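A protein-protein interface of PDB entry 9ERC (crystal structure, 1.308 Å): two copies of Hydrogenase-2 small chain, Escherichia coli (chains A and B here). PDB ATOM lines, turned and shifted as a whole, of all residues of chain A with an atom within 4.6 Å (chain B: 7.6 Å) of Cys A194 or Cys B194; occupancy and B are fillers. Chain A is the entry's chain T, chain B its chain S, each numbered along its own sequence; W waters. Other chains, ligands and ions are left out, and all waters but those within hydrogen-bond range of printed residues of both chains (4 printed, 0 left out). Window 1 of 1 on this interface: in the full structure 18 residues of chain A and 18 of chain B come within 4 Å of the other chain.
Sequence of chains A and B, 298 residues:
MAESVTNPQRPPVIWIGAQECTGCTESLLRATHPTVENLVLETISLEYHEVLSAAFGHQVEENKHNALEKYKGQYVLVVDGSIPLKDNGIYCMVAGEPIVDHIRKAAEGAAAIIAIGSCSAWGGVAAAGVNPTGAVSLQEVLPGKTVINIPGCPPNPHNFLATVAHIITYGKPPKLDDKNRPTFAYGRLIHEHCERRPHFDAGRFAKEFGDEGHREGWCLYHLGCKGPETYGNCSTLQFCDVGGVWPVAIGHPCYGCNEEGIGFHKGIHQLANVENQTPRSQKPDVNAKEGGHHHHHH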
ATOM      1  N   ILE A 190      29.276   7.219   2.643  1.00  0.00           N
ATOM      2  CA  ILE A 190      29.582   6.136   1.722  1.00  0.00           C
ATOM      3  C   ILE A 190      29.474   4.795   2.448  1.00  0.00           C
ATOM      4  O   ILE A 190      28.894   3.865   1.923  1.00  0.00           O
ATOM      5  CB  ILE A 190      30.955   6.374   1.058  1.00  0.00           C
ATOM      6  CG1 ILE A 190      30.888   7.551   0.078  1.00  0.00           C
ATOM      7  CG2 ILE A 190      31.502   5.113   0.410  1.00  0.00           C
ATOM      8  CD1 ILE A 190      32.251   8.039  -0.398  1.00  0.00           C
ATOM      9  N   HIS A 191      30.000   4.711   3.679  1.00  0.00           N
ATOM     10  CA  HIS A 191      29.970   3.498   4.470  1.00  0.00           C
ATOM     11  C   HIS A 191      28.561   3.061   4.852  1.00  0.00           C
ATOM     12  O   HIS A 191      28.387   1.905   5.190  1.00  0.00           O
ATOM     13  CB  HIS A 191      30.793   3.726   5.741  1.00  0.00           C
ATOM     14  CG  HIS A 191      30.970   2.564   6.646  1.00  0.00           C
ATOM     15  ND1 HIS A 191      31.766   1.462   6.443  1.00  0.00           N
ATOM     16  CD2 HIS A 191      30.438   2.421   7.890  1.00  0.00           C
ATOM     17  CE1 HIS A 191      31.686   0.683   7.527  1.00  0.00           C
ATOM     18  NE2 HIS A 191      30.845   1.250   8.408  1.00  0.00           N
ATOM     19  N   GLU A 192      27.592   3.978   4.818  1.00  0.00           N
ATOM     20  CA  GLU A 192      26.201   3.639   5.111  1.00  0.00           C
ATOM     21  C   GLU A 192      25.462   3.253   3.829  1.00  0.00           C
ATOM     22  O   GLU A 192      24.249   3.091   3.861  1.00  0.00           O
ATOM     23  CB  GLU A 192      25.482   4.769   5.842  1.00  0.00           C
ATOM     24  CG  GLU A 192      26.023   4.959   7.253  1.00  0.00           C
ATOM     25  CD  GLU A 192      25.933   3.711   8.107  1.00  0.00           C
ATOM     26  OE1 GLU A 192      24.782   3.138   8.196  1.00  0.00           O
ATOM     27  OE2 GLU A 192      26.968   3.277   8.676  1.00  0.00           O
ATOM     28  N   HIS A 193      26.188   3.094   2.715  1.00  0.00           N
ATOM     29  CA  HIS A 193      25.590   2.528   1.494  1.00  0.00           C
ATOM     30  C   HIS A 193      26.665   1.842   0.640  1.00  0.00           C
ATOM     31  O   HIS A 193      26.662   1.978  -0.594  1.00  0.00           O
ATOM     32  CB  HIS A 193      24.827   3.592   0.709  1.00  0.00           C
ATOM     33  CG  HIS A 193      23.646   3.053  -0.051  1.00  0.00           C
ATOM     34  ND1 HIS A 193      22.355   3.396   0.289  1.00  0.00           N
ATOM     35  CD2 HIS A 193      23.574   2.236  -1.105  1.00  0.00           C
ATOM     36  CE1 HIS A 193      21.516   2.736  -0.529  1.00  0.00           C
ATOM     37  NE2 HIS A 193      22.225   2.026  -1.400  1.00  0.00           N
ATOM     38  N   CYS A 194      27.578   1.111   1.295  1.00  0.00           N
ATOM     39  CA  CYS A 194      28.708   0.455   0.637  1.00  0.00           C
ATOM     40  C   CYS A 194      28.465  -1.051   0.536  1.00  0.00           C
ATOM     41  O   CYS A 194      28.170  -1.706   1.543  1.00  0.00           O
ATOM     42  CB  CYS A 194      30.022   0.749   1.365  1.00  0.00           C
ATOM     43  SG  CYS A 194      31.426  -0.111   0.622  1.00  0.00           S
ATOM     44  N   GLU A 195      28.707  -1.614  -0.666  1.00  0.00           N
ATOM     45  CA  GLU A 195      28.482  -3.023  -0.913  1.00  0.00           C
ATOM     46  C   GLU A 195      29.473  -3.923  -0.184  1.00  0.00           C
ATOM     47  O   GLU A 195      29.255  -5.131  -0.120  1.00  0.00           O
ATOM     48  CB  GLU A 195      28.461  -3.300  -2.419  1.00  0.00           C
ATOM     49  CG  GLU A 195      29.811  -3.155  -3.117  1.00  0.00           C
ATOM     50  CD  GLU A 195      30.172  -1.760  -3.616  1.00  0.00           C
ATOM     51  OE1 GLU A 195      29.523  -0.743  -3.173  1.00  0.00           O
ATOM     52  OE2 GLU A 195      31.125  -1.706  -4.461  1.00  0.00           O
ATOM     53  N   ARG A 196      30.545  -3.368   0.416  1.00  0.00           N
ATOM     54  CA  ARG A 196      31.484  -4.194   1.177  1.00  0.00           C
ATOM     55  C   ARG A 196      31.160  -4.171   2.675  1.00  0.00           C
ATOM     56  O   ARG A 196      31.837  -4.826   3.450  1.00  0.00           O
ATOM     57  CB  ARG A 196      32.915  -3.740   0.919  1.00  0.00           C
ATOM     58  CG  ARG A 196      33.239  -3.830  -0.564  1.00  0.00           C
ATOM     59  CD  ARG A 196      34.681  -3.824  -0.875  1.00  0.00           C
ATOM     60  NE  ARG A 196      34.862  -4.018  -2.307  1.00  0.00           N
ATOM     61  CZ  ARG A 196      36.020  -4.323  -2.871  1.00  0.00           C
ATOM     62  NH1 ARG A 196      37.109  -4.442  -2.127  1.00  0.00           N
ATOM     63  NH2 ARG A 196      36.080  -4.520  -4.180  1.00  0.00           N
ATOM     64  N   ARG A 197      30.073  -3.505   3.054  1.00  0.00           N
ATOM     65  CA  ARG A 197      29.678  -3.467   4.454  1.00  0.00           C
ATOM     66  C   ARG A 197      29.535  -4.873   5.036  1.00  0.00           C
ATOM     67  O   ARG A 197      29.870  -5.105   6.205  1.00  0.00           O
ATOM     68  CB  ARG A 197      28.420  -2.622   4.628  1.00  0.00           C
ATOM     69  CG  ARG A 197      27.921  -2.581   6.059  1.00  0.00           C
ATOM     70  CD  ARG A 197      28.950  -1.916   6.961  1.00  0.00           C
ATOM     71  NE  ARG A 197      28.353  -1.686   8.268  1.00  0.00           N
ATOM     72  CZ  ARG A 197      27.598  -0.659   8.612  1.00  0.00           C
ATOM     73  NH1 ARG A 197      27.598   0.464   7.919  1.00  0.00           N
ATOM     74  NH2 ARG A 197      26.885  -0.731   9.728  1.00  0.00           N
ATOM     75  N   PRO A 198      28.988  -5.876   4.316  1.00  0.00           N
ATOM     76  CA  PRO A 198      28.916  -7.221   4.902  1.00  0.00           C
ATOM     77  C   PRO A 198      30.282  -7.746   5.359  1.00  0.00           C
ATOM     78  O   PRO A 198      30.380  -8.455   6.367  1.00  0.00           O
ATOM     79  CB  PRO A 198      28.339  -8.072   3.761  1.00  0.00           C
ATOM     80  CG  PRO A 198      27.562  -7.085   2.928  1.00  0.00           C
ATOM     81  CD  PRO A 198      28.388  -5.819   2.965  1.00  0.00           C
ATOM     82  N   SER A 235      29.531   4.974  -4.079  1.00  0.00           N
ATOM     83  CA  SER A 235      29.249   3.541  -4.115  1.00  0.00           C
ATOM     84  C   SER A 235      28.008   3.249  -4.938  1.00  0.00           C
ATOM     85  O   SER A 235      27.858   2.100  -5.330  1.00  0.00           O
ATOM     86  CB  SER A 235      29.060   2.968  -2.738  1.00  0.00           C
ATOM     87  OG  SER A 235      28.016   3.634  -2.064  1.00  0.00           O
ATOM     88  N   TRP A 246      34.209   2.493  -9.049  1.00  0.00           N
ATOM     89  CA  TRP A 246      34.540   3.503  -8.063  1.00  0.00           C
ATOM     90  C   TRP A 246      35.783   3.033  -7.336  1.00  0.00           C
ATOM     91  O   TRP A 246      36.227   1.889  -7.520  1.00  0.00           O
ATOM     92  CB  TRP A 246      33.377   3.805  -7.131  1.00  0.00           C
ATOM     93  CG  TRP A 246      32.949   2.767  -6.133  1.00  0.00           C
ATOM     94  CD1 TRP A 246      32.360   1.552  -6.367  1.00  0.00           C
ATOM     95  CD2 TRP A 246      33.006   2.899  -4.695  1.00  0.00           C
ATOM     96  NE1 TRP A 246      32.028   0.949  -5.181  1.00  0.00           N
ATOM     97  CE2 TRP A 246      32.428   1.738  -4.136  1.00  0.00           C
ATOM     98  CE3 TRP A 246      33.468   3.890  -3.822  1.00  0.00           C
ATOM     99  CZ2 TRP A 246      32.324   1.563  -2.754  1.00  0.00           C
ATOM    100  CZ3 TRP A 246      33.367   3.713  -2.458  1.00  0.00           C
ATOM    101  CH2 TRP A 246      32.738   2.593  -1.934  1.00  0.00           C
ATOM    102  N   ARG B 188      29.401 -15.876  -3.978  1.00  0.00           N
ATOM    103  CA  ARG B 188      29.067 -15.135  -2.774  1.00  0.00           C
ATOM    104  C   ARG B 188      27.564 -14.839  -2.744  1.00  0.00           C
ATOM    105  O   ARG B 188      26.949 -14.615  -3.796  1.00  0.00           O
ATOM    106  CB  ARG B 188      29.891 -13.838  -2.742  1.00  0.00           C
ATOM    107  CG  ARG B 188      29.580 -12.916  -1.577  1.00  0.00           C
ATOM    108  CD  ARG B 188      30.596 -11.782  -1.485  1.00  0.00           C
ATOM    109  NE  ARG B 188      31.912 -12.317  -1.181  1.00  0.00           N
ATOM    110  CZ  ARG B 188      33.070 -11.800  -1.595  1.00  0.00           C
ATOM    111  NH1 ARG B 188      33.093 -10.692  -2.299  1.00  0.00           N
ATOM    112  NH2 ARG B 188      34.198 -12.451  -1.374  1.00  0.00           N
ATOM    113  N   LEU B 189      26.959 -14.863  -1.549  1.00  0.00           N
ATOM    114  CA  LEU B 189      25.583 -14.418  -1.380  1.00  0.00           C
ATOM    115  C   LEU B 189      25.456 -12.956  -1.790  1.00  0.00           C
ATOM    116  O   LEU B 189      26.326 -12.139  -1.497  1.00  0.00           O
ATOM    117  CB  LEU B 189      25.127 -14.562   0.081  1.00  0.00           C
ATOM    118  CG  LEU B 189      24.934 -15.996   0.581  1.00  0.00           C
ATOM    119  CD1 LEU B 189      24.779 -16.019   2.093  1.00  0.00           C
ATOM    120  CD2 LEU B 189      23.729 -16.626  -0.067  1.00  0.00           C
ATOM    121  N   ILE B 190      24.331 -12.608  -2.414  1.00  0.00           N
ATOM    122  CA  ILE B 190      24.045 -11.212  -2.728  1.00  0.00           C
ATOM    123  C   ILE B 190      24.087 -10.356  -1.455  1.00  0.00           C
ATOM    124  O   ILE B 190      24.702  -9.290  -1.431  1.00  0.00           O
ATOM    125  CB  ILE B 190      22.721 -11.115  -3.523  1.00  0.00           C
ATOM    126  CG1 ILE B 190      22.898 -11.716  -4.928  1.00  0.00           C
ATOM    127  CG2 ILE B 190      22.227  -9.694  -3.565  1.00  0.00           C
ATOM    128  CD1 ILE B 190      21.588 -11.907  -5.686  1.00  0.00           C
ATOM    129  N   HIS B 191      23.487 -10.847  -0.368  1.00  0.00           N
ATOM    130  CA  HIS B 191      23.445 -10.115   0.893  1.00  0.00           C
ATOM    131  C   HIS B 191      24.824  -9.949   1.521  1.00  0.00           C
ATOM    132  O   HIS B 191      24.972  -9.073   2.380  1.00  0.00           O
ATOM    133  CB  HIS B 191      22.540 -10.881   1.855  1.00  0.00           C
ATOM    134  CG  HIS B 191      22.304 -10.303   3.189  1.00  0.00           C
ATOM    135  ND1 HIS B 191      21.505  -9.222   3.480  1.00  0.00           N
ATOM    136  CD2 HIS B 191      22.767 -10.775   4.386  1.00  0.00           C
ATOM    137  CE1 HIS B 191      21.478  -9.056   4.798  1.00  0.00           C
ATOM    138  NE2 HIS B 191      22.258  -9.950   5.365  1.00  0.00           N
ATOM    139  N   GLU B 192      25.817 -10.761   1.121  1.00  0.00           N
ATOM    140  CA  GLU B 192      27.169 -10.635   1.643  1.00  0.00           C
ATOM    141  C   GLU B 192      27.991  -9.705   0.749  1.00  0.00           C
ATOM    142  O   GLU B 192      29.213  -9.603   0.940  1.00  0.00           O
ATOM    143  CB  GLU B 192      27.837 -11.988   1.828  1.00  0.00           C
ATOM    144  CG  GLU B 192      27.196 -12.790   2.967  1.00  0.00           C
ATOM    145  CD  GLU B 192      27.191 -12.074   4.320  1.00  0.00           C
ATOM    146  OE1 GLU B 192      26.108 -11.963   4.956  1.00  0.00           O
ATOM    147  OE2 GLU B 192      28.256 -11.593   4.744  1.00  0.00           O
ATOM    148  N   HIS B 193      27.322  -9.037  -0.208  1.00  0.00           N
ATOM    149  CA  HIS B 193      27.971  -7.977  -0.989  1.00  0.00           C
ATOM    150  C   HIS B 193      26.948  -6.961  -1.512  1.00  0.00           C
ATOM    151  O   HIS B 193      27.065  -6.477  -2.641  1.00  0.00           O
ATOM    152  CB  HIS B 193      28.846  -8.572  -2.104  1.00  0.00           C
ATOM    153  CG  HIS B 193      30.052  -7.761  -2.451  1.00  0.00           C
ATOM    154  ND1 HIS B 193      31.334  -8.232  -2.217  1.00  0.00           N
ATOM    155  CD2 HIS B 193      30.182  -6.562  -3.013  1.00  0.00           C
ATOM    156  CE1 HIS B 193      32.205  -7.305  -2.611  1.00  0.00           C
ATOM    157  NE2 HIS B 193      31.535  -6.279  -3.115  1.00  0.00           N
ATOM    158  N   CYS B 194      25.999  -6.578  -0.650  1.00  0.00           N
ATOM    159  CA  CYS B 194      24.911  -5.687  -1.019  1.00  0.00           C
ATOM    160  C   CYS B 194      25.114  -4.318  -0.382  1.00  0.00           C
ATOM    161  O   CYS B 194      25.338  -4.216   0.851  1.00  0.00           O
ATOM    162  CB  CYS B 194      23.554  -6.261  -0.596  1.00  0.00           C
ATOM    163  SG  CYS B 194      22.171  -5.130  -0.919  1.00  0.00           S
ATOM    164  N   GLU B 195      24.968  -3.259  -1.201  1.00  0.00           N
ATOM    165  CA  GLU B 195      25.176  -1.894  -0.750  1.00  0.00           C
ATOM    166  C   GLU B 195      24.126  -1.438   0.253  1.00  0.00           C
ATOM    167  O   GLU B 195      24.286  -0.364   0.853  1.00  0.00           O
ATOM    168  CB  GLU B 195      25.273  -0.942  -1.939  1.00  0.00           C
ATOM    169  CG  GLU B 195      23.999  -0.757  -2.751  1.00  0.00           C
ATOM    170  CD  GLU B 195      23.702  -1.763  -3.855  1.00  0.00           C
ATOM    171  OE1 GLU B 195      24.335  -2.877  -3.874  1.00  0.00           O
ATOM    172  OE2 GLU B 195      22.831  -1.420  -4.696  1.00  0.00           O
ATOM    173  N   ARG B 196      23.035  -2.212   0.464  1.00  0.00           N
ATOM    174  CA  ARG B 196      22.037  -1.806   1.438  1.00  0.00           C
ATOM    175  C   ARG B 196      22.257  -2.511   2.773  1.00  0.00           C
ATOM    176  O   ARG B 196      21.511  -2.271   3.720  1.00  0.00           O
ATOM    177  CB  ARG B 196      20.623  -2.038   0.903  1.00  0.00           C
ATOM    178  CG  ARG B 196      20.409  -1.233  -0.365  1.00  0.00           C
ATOM    179  CD  ARG B 196      18.970  -1.134  -0.760  1.00  0.00           C
ATOM    180  NE  ARG B 196      18.888  -0.263  -1.917  1.00  0.00           N
ATOM    181  CZ  ARG B 196      17.777   0.279  -2.373  1.00  0.00           C
ATOM    182  NH1 ARG B 196      16.634   0.064  -1.749  1.00  0.00           N
ATOM    183  NH2 ARG B 196      17.805   1.043  -3.448  1.00  0.00           N
ATOM    184  N   ARG B 197      23.325  -3.289   2.875  1.00  0.00           N
ATOM    185  CA  ARG B 197      23.643  -3.948   4.135  1.00  0.00           C
ATOM    186  C   ARG B 197      23.716  -2.962   5.302  1.00  0.00           C
ATOM    187  O   ARG B 197      23.308  -3.307   6.424  1.00  0.00           O
ATOM    188  CB  ARG B 197      24.940  -4.740   4.023  1.00  0.00           C
ATOM    189  CG  ARG B 197      25.270  -5.509   5.299  1.00  0.00           C
ATOM    190  CD  ARG B 197      24.194  -6.507   5.701  1.00  0.00           C
ATOM    191  NE  ARG B 197      24.672  -7.314   6.810  1.00  0.00           N
ATOM    192  CZ  ARG B 197      25.432  -8.396   6.692  1.00  0.00           C
ATOM    193  NH1 ARG B 197      25.513  -9.077   5.561  1.00  0.00           N
ATOM    194  NH2 ARG B 197      26.041  -8.859   7.767  1.00  0.00           N
ATOM    195  N   PRO B 198      24.286  -1.744   5.165  1.00  0.00           N
ATOM    196  CA  PRO B 198      24.278  -0.837   6.318  1.00  0.00           C
ATOM    197  C   PRO B 198      22.877  -0.561   6.878  1.00  0.00           C
ATOM    198  O   PRO B 198      22.696  -0.371   8.097  1.00  0.00           O
ATOM    199  CB  PRO B 198      24.887   0.448   5.752  1.00  0.00           C
ATOM    200  CG  PRO B 198      25.715  -0.001   4.585  1.00  0.00           C
ATOM    201  CD  PRO B 198      24.942  -1.155   3.981  1.00  0.00           C
ATOM    202  N   HIS B 199      21.886  -0.481   5.970  1.00  0.00           N
ATOM    203  CA  HIS B 199      20.515  -0.198   6.358  1.00  0.00           C
ATOM    204  C   HIS B 199      19.954  -1.416   7.092  1.00  0.00           C
ATOM    205  O   HIS B 199      19.315  -1.263   8.136  1.00  0.00           O
ATOM    206  CB  HIS B 199      19.664   0.175   5.142  1.00  0.00           C
ATOM    207  CG  HIS B 199      20.223   1.321   4.385  1.00  0.00           C
ATOM    208  ND1 HIS B 199      20.483   2.531   5.003  1.00  0.00           N
ATOM    209  CD2 HIS B 199      20.590   1.444   3.117  1.00  0.00           C
ATOM    210  CE1 HIS B 199      20.971   3.362   4.109  1.00  0.00           C
ATOM    211  NE2 HIS B 199      21.075   2.713   2.954  1.00  0.00           N
ATOM    212  N   PHE B 200      20.183  -2.606   6.537  1.00  0.00           N
ATOM    213  CA  PHE B 200      19.837  -3.847   7.215  1.00  0.00           C
ATOM    214  C   PHE B 200      20.387  -3.817   8.647  1.00  0.00           C
ATOM    215  O   PHE B 200      19.677  -4.131   9.612  1.00  0.00           O
ATOM    216  CB  PHE B 200      20.394  -5.030   6.425  1.00  0.00           C
ATOM    217  CG  PHE B 200      20.119  -6.384   7.037  1.00  0.00           C
ATOM    218  CD1 PHE B 200      20.979  -6.939   7.961  1.00  0.00           C
ATOM    219  CD2 PHE B 200      19.016  -7.123   6.638  1.00  0.00           C
ATOM    220  CE1 PHE B 200      20.746  -8.194   8.496  1.00  0.00           C
ATOM    221  CE2 PHE B 200      18.771  -8.374   7.190  1.00  0.00           C
ATOM    222  CZ  PHE B 200      19.634  -8.916   8.114  1.00  0.00           C
ATOM    223  N   CYS B 219      17.018  -0.869   3.126  1.00  0.00           N
ATOM    224  CA  CYS B 219      17.049  -2.297   2.873  1.00  0.00           C
ATOM    225  C   CYS B 219      15.631  -2.817   2.603  1.00  0.00           C
ATOM    226  O   CYS B 219      14.652  -2.335   3.166  1.00  0.00           O
ATOM    227  CB  CYS B 219      17.721  -3.009   4.037  1.00  0.00           C
ATOM    228  SG  CYS B 219      17.535  -4.805   4.108  1.00  0.00           S
ATOM    229  N   LEU B 220      15.559  -3.815   1.714  1.00  0.00           N
ATOM    230  CA  LEU B 220      14.309  -4.392   1.255  1.00  0.00           C
ATOM    231  C   LEU B 220      14.003  -5.748   1.902  1.00  0.00           C
ATOM    232  O   LEU B 220      13.131  -6.477   1.427  1.00  0.00           O
ATOM    233  CB  LEU B 220      14.383  -4.509  -0.271  1.00  0.00           C
ATOM    234  CG  LEU B 220      14.739  -3.220  -1.029  1.00  0.00           C
ATOM    235  CD1 LEU B 220      14.587  -3.436  -2.545  1.00  0.00           C
ATOM    236  CD2 LEU B 220      13.882  -2.069  -0.581  1.00  0.00           C
ATOM    237  N   CYS B 225      13.143  -9.532   0.378  1.00  0.00           N
ATOM    238  CA  CYS B 225      14.406  -9.707  -0.318  1.00  0.00           C
ATOM    239  C   CYS B 225      15.030 -11.065  -0.034  1.00  0.00           C
ATOM    240  O   CYS B 225      15.248 -11.445   1.115  1.00  0.00           O
ATOM    241  CB  CYS B 225      15.360  -8.566   0.006  1.00  0.00           C
ATOM    242  SG  CYS B 225      16.849  -8.627  -1.034  1.00  0.00           S
ATOM    243  N   GLY B 227      18.079 -11.826  -1.100  1.00  0.00           N
ATOM    244  CA  GLY B 227      19.528 -11.684  -1.137  1.00  0.00           C
ATOM    245  C   GLY B 227      20.229 -12.557  -0.086  1.00  0.00           C
ATOM    246  O   GLY B 227      21.303 -13.117  -0.323  1.00  0.00           O
ATOM    247  N   SER B 235      24.500  -7.544  -7.318  1.00  0.00           N
ATOM    248  CA  SER B 235      24.762  -6.278  -6.663  1.00  0.00           C
ATOM    249  C   SER B 235      26.051  -5.647  -7.182  1.00  0.00           C
ATOM    250  O   SER B 235      26.216  -4.460  -6.972  1.00  0.00           O
ATOM    251  CB  SER B 235      24.820  -6.430  -5.155  1.00  0.00           C
ATOM    252  OG  SER B 235      25.884  -7.320  -4.811  1.00  0.00           O
ATOM    253  N   THR B 236      26.958  -6.435  -7.784  1.00  0.00           N
ATOM    254  CA  THR B 236      28.248  -5.904  -8.213  1.00  0.00           C
ATOM    255  C   THR B 236      28.291  -5.748  -9.733  1.00  0.00           C
ATOM    256  O   THR B 236      28.377  -4.637 -10.245  1.00  0.00           O
ATOM    257  CB  THR B 236      29.403  -6.771  -7.704  1.00  0.00           C
ATOM    258  OG1 THR B 236      29.140  -8.152  -7.923  1.00  0.00           O
ATOM    259  CG2 THR B 236      29.639  -6.591  -6.220  1.00  0.00           C
ATOM    260  N   TRP B 246      20.110  -2.979 -10.905  1.00  0.00           N
ATOM    261  CA  TRP B 246      19.741  -4.331 -10.516  1.00  0.00           C
ATOM    262  C   TRP B 246      18.437  -4.225  -9.730  1.00  0.00           C
ATOM    263  O   TRP B 246      18.014  -3.112  -9.378  1.00  0.00           O
ATOM    264  CB  TRP B 246      20.849  -5.051  -9.743  1.00  0.00           C
ATOM    265  CG  TRP B 246      21.191  -4.589  -8.355  1.00  0.00           C
ATOM    266  CD1 TRP B 246      21.784  -3.420  -7.964  1.00  0.00           C
ATOM    267  CD2 TRP B 246      21.030  -5.366  -7.143  1.00  0.00           C
ATOM    268  NE1 TRP B 246      22.038  -3.440  -6.615  1.00  0.00           N
ATOM    269  CE2 TRP B 246      21.560  -4.609  -6.078  1.00  0.00           C
ATOM    270  CE3 TRP B 246      20.521  -6.634  -6.864  1.00  0.00           C
ATOM    271  CZ2 TRP B 246      21.559  -5.088  -4.764  1.00  0.00           C
ATOM    272  CZ3 TRP B 246      20.524  -7.114  -5.571  1.00  0.00           C
ATOM    273  CH2 TRP B 246      21.086  -6.367  -4.534  1.00  0.00           C
ATOM    274  N   VAL B 248      17.216  -4.643  -6.673  1.00  0.00           N
ATOM    275  CA  VAL B 248      17.202  -3.940  -5.403  1.00  0.00           C
ATOM    276  C   VAL B 248      17.494  -2.463  -5.607  1.00  0.00           C
ATOM    277  O   VAL B 248      16.817  -1.615  -5.028  1.00  0.00           O
ATOM    278  CB  VAL B 248      18.201  -4.586  -4.436  1.00  0.00           C
ATOM    279  CG1 VAL B 248      18.490  -3.670  -3.254  1.00  0.00           C
ATOM    280  CG2 VAL B 248      17.666  -5.932  -3.959  1.00  0.00           C
ATOM    281  N   ALA B 249      18.464  -2.139  -6.468  1.00  0.00           N
ATOM    282  CA  ALA B 249      18.770  -0.726  -6.702  1.00  0.00           C
ATOM    283  C   ALA B 249      17.565   0.015  -7.287  1.00  0.00           C
ATOM    284  O   ALA B 249      17.384   1.217  -7.079  1.00  0.00           O
ATOM    285  CB  ALA B 249      19.960  -0.583  -7.621  1.00  0.00           C
HETATM  286  O   HOH W   1      24.570   0.943   9.671  1.00  0.00           O
HETATM  287  O   HOH W   2      32.732  -3.932  -4.332  1.00  0.00           O
HETATM  288  O   HOH W   3      21.177   0.538  -3.683  1.00  0.00           O
HETATM  289  O   HOH W   4      28.480 -10.321   7.014  1.00  0.00           O
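NE2 of His B199 lies close to O of Glu A192 (3.3 Å). NE2 of His B199 is in hydrogen-bond range of ND1 of His A193, 3.0 Å away.
NH1 of Arg B197 lies within hydrogen-bond range of O of His B191, at 3.2 Å. The side-chain carboxylate of Glu B192 is in salt-bridge range of the guanidinium group of Arg B197 (3.0 Å). The backbone NH of His B191 is in hydrogen-bond range of the backbone carbonyl oxygen of Gly B227 (3.2 Å). NH2 of Arg B196 lies within hydrogen-bond range of O of Val B248 (3.2 Å). NH1 of Arg A197 lies within hydrogen-bond range of O of His A191 (3.2 Å). SG of Cys B194 lies close to N of Arg B196.
Among the printed residues, merely in contact across the chains: His A193 with Glu B195 (3.2 Å), Glu A195 with His B193 (3.2 Å), Pro A198 with His B191 (3.3 Å), Glu A192 with Pro B198 (3.3 Å), Pro A198 with Glu B192 (3.3 Å), His A191 with Pro B198 (3.3 Å), Arg A197 with Pro B198 (3.5 Å), Glu A195 with Glu B195 (3.5 Å), Pro A198 with Arg B197 (3.5 Å), Glu A195 with Cys B194 (3.6 Å), Cys A194 with Glu B195 (3.6 Å), His A193 with Pro B198 (3.6 Å), Pro A198 with His B193 (3.7 Å), Cys A194 with Cys B194 (3.8 Å), His A193 with Arg B196 (3.9 Å), Arg A196 with His B193 (3.9 Å), Pro A198 with Cys B194 (3.9 Å) and Cys A194 with Pro B198 (3.9 Å).
Of the printed residues of chain B, Cys A194 touches Cys B194, Glu B195 and Pro B198. Of the printed residues of chain A, His B193 touches Glu A195, Arg A196 and Pro A198. Cys B194 touches three residues of chain A. Printed residues of chain A within 4 Å of Glu B195: His A193 (3.2 Å), Cys A194 (3.6 Å) and Glu A195 (3.5 Å). Of the printed residues of chain A, Arg B196 touches His A193 (3.9 Å). Gly B227 touches none of the printed residues of chain A. Ser B235 touches none of the printed residues of chain A. The nearest residue of chain B that does not touch Cys A194 is Arg B197 (5.1 Å).
Printed residues of chain B that touch a printed residue of chain A: His B191, Glu B192, His B193, Cys B194, Glu B195, Arg B196, Arg B197, Pro B198 and His B199. Hydrophobic or aromatic side chains of chain B that line the printed part of chain A: His B193, Pro B198 and His B199. Along chain B the printed residues that touch a printed residue of chain A span positions 191 to 199. Printed residues of chain A that touch a printed residue of chain B: His A191, Glu A192, His A193, Cys A194, Glu A195, Arg A196, Arg A197 and Pro A198. Hydrophobic or aromatic side chains of chain A within 4 Å of the printed part of chain B: His A193 and Pro A198. Among the printed residues, 20 pairs touch across the chains. Among the printed residues, no Asp or Glu carboxylate lies within 4 Å of a Lys or Arg side-chain nitrogen of the other chain.
His A191 touches Pro B198, and with the chains exchanged Pro A198 touches His B191. His A193 touches Glu B195, and with the chains exchanged Glu A195 touches His B193. Cys A194 touches its own counterpart, Cys B194. Glu A195 touches its own counterpart, Glu B195. Positions printed for both chains: 190, 191, 192, 193, 194, 195, 196, 197, 198, 235 and 246. Of the 20 pairs that touch across the chains among the printed residues, 18 have their exchanged pair printed and touching as well.
Water W4 lies within hydrogen-bond range of OE2 of Glu B192 (2.6 Å), O of Pro A198 (2.7 Å) and NH2 of Arg B197 (2.9 Å). Water W1 lies within hydrogen-bond range of the side-chain carboxylate (OE1) of Glu A192 (2.7 Å), the backbone carbonyl oxygen (O) of Pro B198 (2.8 Å) and the guanidinium group (NH2) of Arg A197 (2.9 Å). Water W2 lies within hydrogen-bond range of the side-chain carboxylate (OE2) of Glu A195, a ring nitrogen (NE2) of His B193 and the guanidinium group (NE) of Arg A196. Water W3 lies within hydrogen-bond range of the side-chain carboxylate (OE2) of Glu B195, a ring nitrogen (NE2) of His A193 and the guanidinium group (NE) of Arg B196.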
